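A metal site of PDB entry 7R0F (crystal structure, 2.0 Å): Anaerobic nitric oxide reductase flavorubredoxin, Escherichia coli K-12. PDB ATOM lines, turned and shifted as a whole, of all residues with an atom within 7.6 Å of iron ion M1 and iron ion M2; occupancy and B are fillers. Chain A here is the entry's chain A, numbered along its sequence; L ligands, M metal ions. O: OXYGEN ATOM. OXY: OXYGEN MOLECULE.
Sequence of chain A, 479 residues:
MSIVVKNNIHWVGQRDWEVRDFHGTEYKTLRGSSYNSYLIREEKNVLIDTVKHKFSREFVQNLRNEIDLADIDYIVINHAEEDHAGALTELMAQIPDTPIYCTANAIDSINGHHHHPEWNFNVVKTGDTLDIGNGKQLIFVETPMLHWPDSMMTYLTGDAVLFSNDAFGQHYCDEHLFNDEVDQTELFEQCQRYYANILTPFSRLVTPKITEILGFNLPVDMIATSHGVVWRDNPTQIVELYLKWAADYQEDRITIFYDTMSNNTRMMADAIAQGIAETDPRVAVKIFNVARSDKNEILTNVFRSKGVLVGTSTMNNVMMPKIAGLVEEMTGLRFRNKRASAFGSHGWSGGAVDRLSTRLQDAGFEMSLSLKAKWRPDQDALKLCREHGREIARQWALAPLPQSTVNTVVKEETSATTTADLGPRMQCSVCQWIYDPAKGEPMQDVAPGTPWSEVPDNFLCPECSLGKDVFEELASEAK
Of the 24 residues printed, 4 come within 4 Å of iron ion M2.
The nearest printed residue that does not touch iron ion M2 is Ser 226 (4.3 Å).
A ring nitrogen (NE2) of His 147 lies close to an oxygen (O2) of OXY L2 (3.4 Å).
The side-chain hydroxyl (OH) of Tyr 194 lies within hydrogen-bond range of an oxygen (O1) of OXY L2, 2.8 Å away.
A ring nitrogen (NE2) of His 23 is in hydrogen-bond range of an oxygen (O2) of OXY L2 (3.4 Å).
Iron ion M2 is bound by O of O L1, at 1.9 Å.
Iron ion M2 is bound by a ring nitrogen (NE2) of His 84, 2.1 Å away.
The side-chain carboxylate (OD1) of Asp 166 is bound to iron ion M2.
NE2 of His 227 is bound to iron ion M2, at 2.4 Å.
OD2 of Asp 83 is bound to iron ion M2 (2.4 Å).
A ring nitrogen (NE2) of His 23 sits at hydrogen-bond distance from the side-chain carboxylate (OE2) of Glu 81.
The side-chain hydroxyl (OG) of Ser 226 sits close to a ring nitrogen (NE2) of His 84 (3.4 Å).
The backbone NH (N) of Asp 166 is in hydrogen-bond range of the side-chain hydroxyl (OG) of Ser 226, 3.2 Å away.
The backbone NH (N) of His 147 lies within hydrogen-bond range of the side-chain hydroxyl (OG) of Ser 151 (3.4 Å).
The backbone carbonyl oxygen (O) of Ser 34 sits at hydrogen-bond distance from a ring nitrogen (ND1) of His 227 (2.7 Å).
OG of Ser 33 sits at hydrogen-bond distance from ND1 of His 227, 3.4 Å away.
ND1 of His 79 lies within hydrogen-bond range of OG of Ser 151, at 3.4 Å.
ND1 of His 79 lies within hydrogen-bond range of OD1 of Asp 150 (2.9 Å).
An oxygen (O) of O L1 is bound to iron ion M1 (1.9 Å).
Iron ion M1 is bound by the side-chain carboxylate (OE1) of Glu 81 (2.0 Å).
OD2 of Asp 166 binds iron ion M1 (2.1 Å).
Iron ion M1 is bound by a ring nitrogen (NE2) of His 147 (2.2 Å).
NE2 of His 79 is bound to iron ion M1, at 2.5 Å.
Iron ion M1 has five donor atoms within binding distance.
Slightly farther from iron ion M1 lies O2 of OXY L2 (2.8 Å).
Of the 24 residues printed, 4 come within 4 Å of iron ion M1.
The nearest printed residue that does not touch iron ion M1 is His 84 (4.3 Å).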
ATOM      1  N   PHE A  22     -11.448  23.278   9.249  1.00  0.00           N
ATOM      2  CA  PHE A  22     -10.509  23.766  10.255  1.00  0.00           C
ATOM      3  C   PHE A  22      -9.866  25.066   9.779  1.00  0.00           C
ATOM      4  O   PHE A  22      -9.727  25.292   8.572  1.00  0.00           O
ATOM      5  CB  PHE A  22      -9.430  22.723  10.554  1.00  0.00           C
ATOM      6  CG  PHE A  22      -9.670  21.943  11.806  1.00  0.00           C
ATOM      7  CD1 PHE A  22     -10.580  20.898  11.830  1.00  0.00           C
ATOM      8  CD2 PHE A  22      -8.981  22.254  12.975  1.00  0.00           C
ATOM      9  CE1 PHE A  22     -10.806  20.183  12.997  1.00  0.00           C
ATOM     10  CE2 PHE A  22      -9.205  21.535  14.134  1.00  0.00           C
ATOM     11  CZ  PHE A  22     -10.115  20.503  14.138  1.00  0.00           C
ATOM     12  N   HIS A  23      -9.493  25.924  10.730  1.00  0.00           N
ATOM     13  CA  HIS A  23      -8.899  27.219  10.436  1.00  0.00           C
ATOM     14  C   HIS A  23      -9.780  28.007   9.468  1.00  0.00           C
ATOM     15  O   HIS A  23      -9.320  28.468   8.419  1.00  0.00           O
ATOM     16  CB  HIS A  23      -7.494  27.052   9.850  1.00  0.00           C
ATOM     17  CG  HIS A  23      -6.551  26.319  10.746  1.00  0.00           C
ATOM     18  ND1 HIS A  23      -5.528  25.522  10.259  1.00  0.00           N
ATOM     19  CD2 HIS A  23      -6.473  26.249  12.097  1.00  0.00           C
ATOM     20  CE1 HIS A  23      -4.866  24.998  11.280  1.00  0.00           C
ATOM     21  NE2 HIS A  23      -5.416  25.425  12.402  1.00  0.00           N
ATOM     22  N   SER A  33     -11.900  14.409  12.661  1.00  0.00           N
ATOM     23  CA  SER A  33     -10.725  14.532  13.509  1.00  0.00           C
ATOM     24  C   SER A  33     -11.049  14.123  14.933  1.00  0.00           C
ATOM     25  O   SER A  33     -12.177  13.729  15.240  1.00  0.00           O
ATOM     26  CB  SER A  33     -10.180  15.964  13.495  1.00  0.00           C
ATOM     27  OG  SER A  33      -9.034  16.088  14.320  1.00  0.00           O
ATOM     28  N   SER A  34     -10.045  14.190  15.802  1.00  0.00           N
ATOM     29  CA  SER A  34     -10.258  13.961  17.218  1.00  0.00           C
ATOM     30  C   SER A  34      -9.477  14.978  18.024  1.00  0.00           C
ATOM     31  O   SER A  34      -8.481  15.525  17.551  1.00  0.00           O
ATOM     32  CB  SER A  34      -9.840  12.535  17.608  1.00  0.00           C
ATOM     33  OG  SER A  34      -8.437  12.369  17.512  1.00  0.00           O
ATOM     34  N   TYR A  35      -9.943  15.252  19.234  1.00  0.00           N
ATOM     35  CA  TYR A  35      -9.242  16.143  20.126  1.00  0.00           C
ATOM     36  C   TYR A  35      -8.845  15.356  21.358  1.00  0.00           C
ATOM     37  O   TYR A  35      -9.684  15.076  22.217  1.00  0.00           O
ATOM     38  CB  TYR A  35     -10.121  17.346  20.477  1.00  0.00           C
ATOM     39  CG  TYR A  35     -10.865  17.881  19.285  1.00  0.00           C
ATOM     40  CD1 TYR A  35     -10.200  18.575  18.279  1.00  0.00           C
ATOM     41  CD2 TYR A  35     -12.232  17.678  19.152  1.00  0.00           C
ATOM     42  CE1 TYR A  35     -10.878  19.059  17.179  1.00  0.00           C
ATOM     43  CE2 TYR A  35     -12.923  18.162  18.047  1.00  0.00           C
ATOM     44  CZ  TYR A  35     -12.237  18.850  17.066  1.00  0.00           C
ATOM     45  OH  TYR A  35     -12.909  19.328  15.971  1.00  0.00           O
ATOM     46  N   HIS A  79      -0.343  23.587  24.228  1.00  0.00           N
ATOM     47  CA  HIS A  79      -0.692  24.405  23.068  1.00  0.00           C
ATOM     48  C   HIS A  79      -2.077  25.002  23.299  1.00  0.00           C
ATOM     49  O   HIS A  79      -3.019  24.285  23.627  1.00  0.00           O
ATOM     50  CB  HIS A  79      -0.654  23.535  21.809  1.00  0.00           C
ATOM     51  CG  HIS A  79      -0.955  24.277  20.541  1.00  0.00           C
ATOM     52  ND1 HIS A  79      -0.392  25.496  20.233  1.00  0.00           N
ATOM     53  CD2 HIS A  79      -1.746  23.951  19.491  1.00  0.00           C
ATOM     54  CE1 HIS A  79      -0.840  25.893  19.062  1.00  0.00           C
ATOM     55  NE2 HIS A  79      -1.658  24.974  18.588  1.00  0.00           N
ATOM     56  N   ALA A  80      -2.191  26.310  23.118  1.00  0.00           N
ATOM     57  CA  ALA A  80      -3.412  27.017  23.513  1.00  0.00           C
ATOM     58  C   ALA A  80      -4.323  27.362  22.338  1.00  0.00           C
ATOM     59  O   ALA A  80      -5.119  28.295  22.432  1.00  0.00           O
ATOM     60  CB  ALA A  80      -3.066  28.277  24.281  1.00  0.00           C
ATOM     61  N   GLU A  81      -4.221  26.614  21.249  1.00  0.00           N
ATOM     62  CA  GLU A  81      -5.169  26.778  20.148  1.00  0.00           C
ATOM     63  C   GLU A  81      -6.531  26.249  20.611  1.00  0.00           C
ATOM     64  O   GLU A  81      -6.596  25.365  21.462  1.00  0.00           O
ATOM     65  CB  GLU A  81      -4.684  26.057  18.887  1.00  0.00           C
ATOM     66  CG  GLU A  81      -5.467  26.421  17.625  1.00  0.00           C
ATOM     67  CD  GLU A  81      -4.737  26.050  16.351  1.00  0.00           C
ATOM     68  OE1 GLU A  81      -3.614  25.508  16.433  1.00  0.00           O
ATOM     69  OE2 GLU A  81      -5.286  26.314  15.261  1.00  0.00           O
ATOM     70  N   GLU A  82      -7.594  26.798  20.042  1.00  0.00           N
ATOM     71  CA  GLU A  82      -8.958  26.547  20.519  1.00  0.00           C
ATOM     72  C   GLU A  82      -9.359  25.068  20.553  1.00  0.00           C
ATOM     73  O   GLU A  82     -10.262  24.690  21.302  1.00  0.00           O
ATOM     74  CB  GLU A  82      -9.970  27.303  19.645  1.00  0.00           C
ATOM     75  CG  GLU A  82     -10.121  26.754  18.242  1.00  0.00           C
ATOM     76  CD  GLU A  82     -11.152  27.511  17.422  1.00  0.00           C
ATOM     77  OE1 GLU A  82     -11.768  28.452  17.958  1.00  0.00           O
ATOM     78  OE2 GLU A  82     -11.347  27.162  16.236  1.00  0.00           O
ATOM     79  N   ASP A  83      -8.699  24.238  19.757  1.00  0.00           N
ATOM     80  CA  ASP A  83      -9.084  22.833  19.679  1.00  0.00           C
ATOM     81  C   ASP A  83      -8.412  21.985  20.754  1.00  0.00           C
ATOM     82  O   ASP A  83      -8.599  20.775  20.826  1.00  0.00           O
ATOM     83  CB  ASP A  83      -8.745  22.272  18.291  1.00  0.00           C
ATOM     84  CG  ASP A  83      -7.289  22.444  17.922  1.00  0.00           C
ATOM     85  OD1 ASP A  83      -6.655  23.390  18.447  1.00  0.00           O
ATOM     86  OD2 ASP A  83      -6.769  21.642  17.118  1.00  0.00           O
ATOM     87  N   HIS A  84      -7.627  22.639  21.613  1.00  0.00           N
ATOM     88  CA  HIS A  84      -6.965  21.935  22.707  1.00  0.00           C
ATOM     89  C   HIS A  84      -7.184  22.657  24.040  1.00  0.00           C
ATOM     90  O   HIS A  84      -7.170  22.027  25.096  1.00  0.00           O
ATOM     91  CB  HIS A  84      -5.467  21.782  22.429  1.00  0.00           C
ATOM     92  CG  HIS A  84      -5.165  21.270  21.060  1.00  0.00           C
ATOM     93  ND1 HIS A  84      -5.672  20.065  20.593  1.00  0.00           N
ATOM     94  CD2 HIS A  84      -4.427  21.777  20.048  1.00  0.00           C
ATOM     95  CE1 HIS A  84      -5.250  19.873  19.353  1.00  0.00           C
ATOM     96  NE2 HIS A  84      -4.489  20.890  19.009  1.00  0.00           N
ATOM     97  N   LEU A 146       6.398  25.490  16.390  1.00  0.00           N
ATOM     98  CA  LEU A 146       6.005  24.158  15.907  1.00  0.00           C
ATOM     99  C   LEU A 146       4.681  23.722  16.536  1.00  0.00           C
ATOM    100  O   LEU A 146       4.653  22.840  17.387  1.00  0.00           O
ATOM    101  CB  LEU A 146       7.094  23.137  16.221  1.00  0.00           C
ATOM    102  CG  LEU A 146       8.437  23.314  15.513  1.00  0.00           C
ATOM    103  CD1 LEU A 146       9.473  22.348  16.057  1.00  0.00           C
ATOM    104  CD2 LEU A 146       8.280  23.138  14.001  1.00  0.00           C
ATOM    105  N   HIS A 147       3.568  24.339  16.104  1.00  0.00           N
ATOM    106  CA  HIS A 147       3.577  25.320  15.025  1.00  0.00           C
ATOM    107  C   HIS A 147       3.268  26.725  15.537  1.00  0.00           C
ATOM    108  O   HIS A 147       3.137  27.669  14.749  1.00  0.00           O
ATOM    109  CB  HIS A 147       2.567  24.922  13.939  1.00  0.00           C
ATOM    110  CG  HIS A 147       1.153  24.924  14.414  1.00  0.00           C
ATOM    111  ND1 HIS A 147       0.296  25.998  14.226  1.00  0.00           N
ATOM    112  CD2 HIS A 147       0.423  23.982  15.068  1.00  0.00           C
ATOM    113  CE1 HIS A 147      -0.880  25.712  14.744  1.00  0.00           C
ATOM    114  NE2 HIS A 147      -0.827  24.501  15.260  1.00  0.00           N
ATOM    115  N   TRP A 148       3.158  26.863  16.851  1.00  0.00           N
ATOM    116  CA  TRP A 148       2.910  28.163  17.474  1.00  0.00           C
ATOM    117  C   TRP A 148       4.045  28.513  18.439  1.00  0.00           C
ATOM    118  O   TRP A 148       4.792  27.629  18.864  1.00  0.00           O
ATOM    119  CB  TRP A 148       1.576  28.157  18.229  1.00  0.00           C
ATOM    120  CG  TRP A 148       0.384  28.553  17.399  1.00  0.00           C
ATOM    121  CD1 TRP A 148       0.311  28.584  16.037  1.00  0.00           C
ATOM    122  CD2 TRP A 148      -0.894  28.978  17.886  1.00  0.00           C
ATOM    123  NE1 TRP A 148      -0.932  29.000  15.644  1.00  0.00           N
ATOM    124  CE2 TRP A 148      -1.700  29.249  16.758  1.00  0.00           C
ATOM    125  CE3 TRP A 148      -1.441  29.155  19.162  1.00  0.00           C
ATOM    126  CZ2 TRP A 148      -3.017  29.678  16.871  1.00  0.00           C
ATOM    127  CZ3 TRP A 148      -2.742  29.580  19.271  1.00  0.00           C
ATOM    128  CH2 TRP A 148      -3.521  29.847  18.131  1.00  0.00           C
ATOM    129  N   ASP A 150       3.730  29.176  21.445  1.00  0.00           N
ATOM    130  CA  ASP A 150       3.412  28.614  22.756  1.00  0.00           C
ATOM    131  C   ASP A 150       3.595  27.105  22.816  1.00  0.00           C
ATOM    132  O   ASP A 150       3.485  26.503  23.883  1.00  0.00           O
ATOM    133  CB  ASP A 150       1.975  28.981  23.146  1.00  0.00           C
ATOM    134  CG  ASP A 150       0.926  28.254  22.296  1.00  0.00           C
ATOM    135  OD1 ASP A 150       1.282  27.665  21.264  1.00  0.00           O
ATOM    136  OD2 ASP A 150      -0.261  28.280  22.679  1.00  0.00           O
ATOM    137  N   SER A 151       3.873  26.498  21.667  1.00  0.00           N
ATOM    138  CA  SER A 151       3.882  25.047  21.541  1.00  0.00           C
ATOM    139  C   SER A 151       4.986  24.375  22.360  1.00  0.00           C
ATOM    140  O   SER A 151       6.120  24.868  22.413  1.00  0.00           O
ATOM    141  CB  SER A 151       4.005  24.644  20.075  1.00  0.00           C
ATOM    142  OG  SER A 151       2.897  25.108  19.321  1.00  0.00           O
ATOM    143  N   ASN A 165       1.329  16.714  21.390  1.00  0.00           N
ATOM    144  CA  ASN A 165       0.265  17.623  20.969  1.00  0.00           C
ATOM    145  C   ASN A 165       0.044  17.555  19.441  1.00  0.00           C
ATOM    146  O   ASN A 165      -0.247  16.488  18.907  1.00  0.00           O
ATOM    147  CB  ASN A 165       0.560  19.052  21.405  1.00  0.00           C
ATOM    148  CG  ASN A 165      -0.671  19.944  21.376  1.00  0.00           C
ATOM    149  OD1 ASN A 165      -0.882  20.689  20.423  1.00  0.00           O
ATOM    150  ND2 ASN A 165      -1.479  19.865  22.431  1.00  0.00           N
ATOM    151  N   ASP A 166       0.183  18.695  18.768  1.00  0.00           N
ATOM    152  CA  ASP A 166      -0.062  18.765  17.318  1.00  0.00           C
ATOM    153  C   ASP A 166       0.943  17.953  16.502  1.00  0.00           C
ATOM    154  O   ASP A 166       0.593  17.375  15.474  1.00  0.00           O
ATOM    155  CB  ASP A 166      -0.039  20.225  16.848  1.00  0.00           C
ATOM    156  CG  ASP A 166      -1.392  20.891  16.963  1.00  0.00           C
ATOM    157  OD1 ASP A 166      -2.397  20.181  17.151  1.00  0.00           O
ATOM    158  OD2 ASP A 166      -1.457  22.132  16.840  1.00  0.00           O
ATOM    159  N   ALA A 167       2.192  17.938  16.959  1.00  0.00           N
ATOM    160  CA  ALA A 167       3.258  17.243  16.240  1.00  0.00           C
ATOM    161  C   ALA A 167       2.966  15.758  16.074  1.00  0.00           C
ATOM    162  O   ALA A 167       2.470  15.113  17.001  1.00  0.00           O
ATOM    163  CB  ALA A 167       4.585  17.444  16.950  1.00  0.00           C
ATOM    164  N   HIS A 171      -5.580  14.678  11.291  1.00  0.00           N
ATOM    165  CA  HIS A 171      -7.028  14.759  11.410  1.00  0.00           C
ATOM    166  C   HIS A 171      -7.659  13.498  10.833  1.00  0.00           C
ATOM    167  O   HIS A 171      -7.980  13.433   9.648  1.00  0.00           O
ATOM    168  CB  HIS A 171      -7.557  16.018  10.712  1.00  0.00           C
ATOM    169  CG  HIS A 171      -7.074  17.292  11.326  1.00  0.00           C
ATOM    170  ND1 HIS A 171      -7.357  17.642  12.630  1.00  0.00           N
ATOM    171  CD2 HIS A 171      -6.325  18.298  10.824  1.00  0.00           C
ATOM    172  CE1 HIS A 171      -6.804  18.808  12.905  1.00  0.00           C
ATOM    173  NE2 HIS A 171      -6.173  19.228  11.821  1.00  0.00           N
ATOM    174  N   TYR A 194      -1.636  16.686   6.676  1.00  0.00           N
ATOM    175  CA  TYR A 194      -1.471  17.589   7.806  1.00  0.00           C
ATOM    176  C   TYR A 194      -0.154  18.346   7.728  1.00  0.00           C
ATOM    177  O   TYR A 194      -0.137  19.573   7.841  1.00  0.00           O
ATOM    178  CB  TYR A 194      -1.554  16.818   9.122  1.00  0.00           C
ATOM    179  CG  TYR A 194      -1.475  17.715  10.347  1.00  0.00           C
ATOM    180  CD1 TYR A 194      -2.606  18.369  10.808  1.00  0.00           C
ATOM    181  CD2 TYR A 194      -0.278  17.894  11.022  1.00  0.00           C
ATOM    182  CE1 TYR A 194      -2.533  19.193  11.928  1.00  0.00           C
ATOM    183  CE2 TYR A 194      -0.202  18.713  12.134  1.00  0.00           C
ATOM    184  CZ  TYR A 194      -1.340  19.357  12.574  1.00  0.00           C
ATOM    185  OH  TYR A 194      -1.272  20.169  13.686  1.00  0.00           O
ATOM    186  N   ILE A 198       0.252  22.464   6.971  1.00  0.00           N
ATOM    187  CA  ILE A 198       0.431  23.164   8.243  1.00  0.00           C
ATOM    188  C   ILE A 198       1.897  23.381   8.625  1.00  0.00           C
ATOM    189  O   ILE A 198       2.278  24.488   9.007  1.00  0.00           O
ATOM    190  CB  ILE A 198      -0.266  22.405   9.387  1.00  0.00           C
ATOM    191  CG1 ILE A 198      -1.744  22.199   9.080  1.00  0.00           C
ATOM    192  CG2 ILE A 198      -0.089  23.148  10.705  1.00  0.00           C
ATOM    193  CD1 ILE A 198      -2.506  23.485   8.846  1.00  0.00           C
ATOM    194  N   SER A 226      -2.299  15.147  19.947  1.00  0.00           N
ATOM    195  CA  SER A 226      -3.559  15.799  20.288  1.00  0.00           C
ATOM    196  C   SER A 226      -4.604  15.573  19.206  1.00  0.00           C
ATOM    197  O   SER A 226      -5.774  15.942  19.373  1.00  0.00           O
ATOM    198  CB  SER A 226      -3.338  17.300  20.505  1.00  0.00           C
ATOM    199  OG  SER A 226      -2.925  17.922  19.304  1.00  0.00           O
ATOM    200  N   HIS A 227      -4.187  14.976  18.090  1.00  0.00           N
ATOM    201  CA  HIS A 227      -5.104  14.701  16.988  1.00  0.00           C
ATOM    202  C   HIS A 227      -4.872  13.302  16.419  1.00  0.00           C
ATOM    203  O   HIS A 227      -3.748  12.929  16.066  1.00  0.00           O
ATOM    204  CB  HIS A 227      -4.947  15.732  15.871  1.00  0.00           C
ATOM    205  CG  HIS A 227      -5.448  17.094  16.228  1.00  0.00           C
ATOM    206  ND1 HIS A 227      -6.772  17.361  16.474  1.00  0.00           N
ATOM    207  CD2 HIS A 227      -4.795  18.275  16.370  1.00  0.00           C
ATOM    208  CE1 HIS A 227      -6.926  18.648  16.746  1.00  0.00           C
ATOM    209  NE2 HIS A 227      -5.741  19.222  16.694  1.00  0.00           N
HETATM  210  O     O L   1      -4.140  23.007  16.988  1.00  0.00           O
HETATM  211  O1  OXY L   2      -3.316  21.909  14.288  1.00  0.00           O
HETATM  212  O2  OXY L   2      -3.684  23.040  14.135  1.00  0.00           O
HETATM  213 FE    FE M   1      -2.525  23.870  16.573  1.00  0.00          FE
HETATM  214 FE    FE M   2      -4.448  21.166  16.972  1.00  0.00          FE
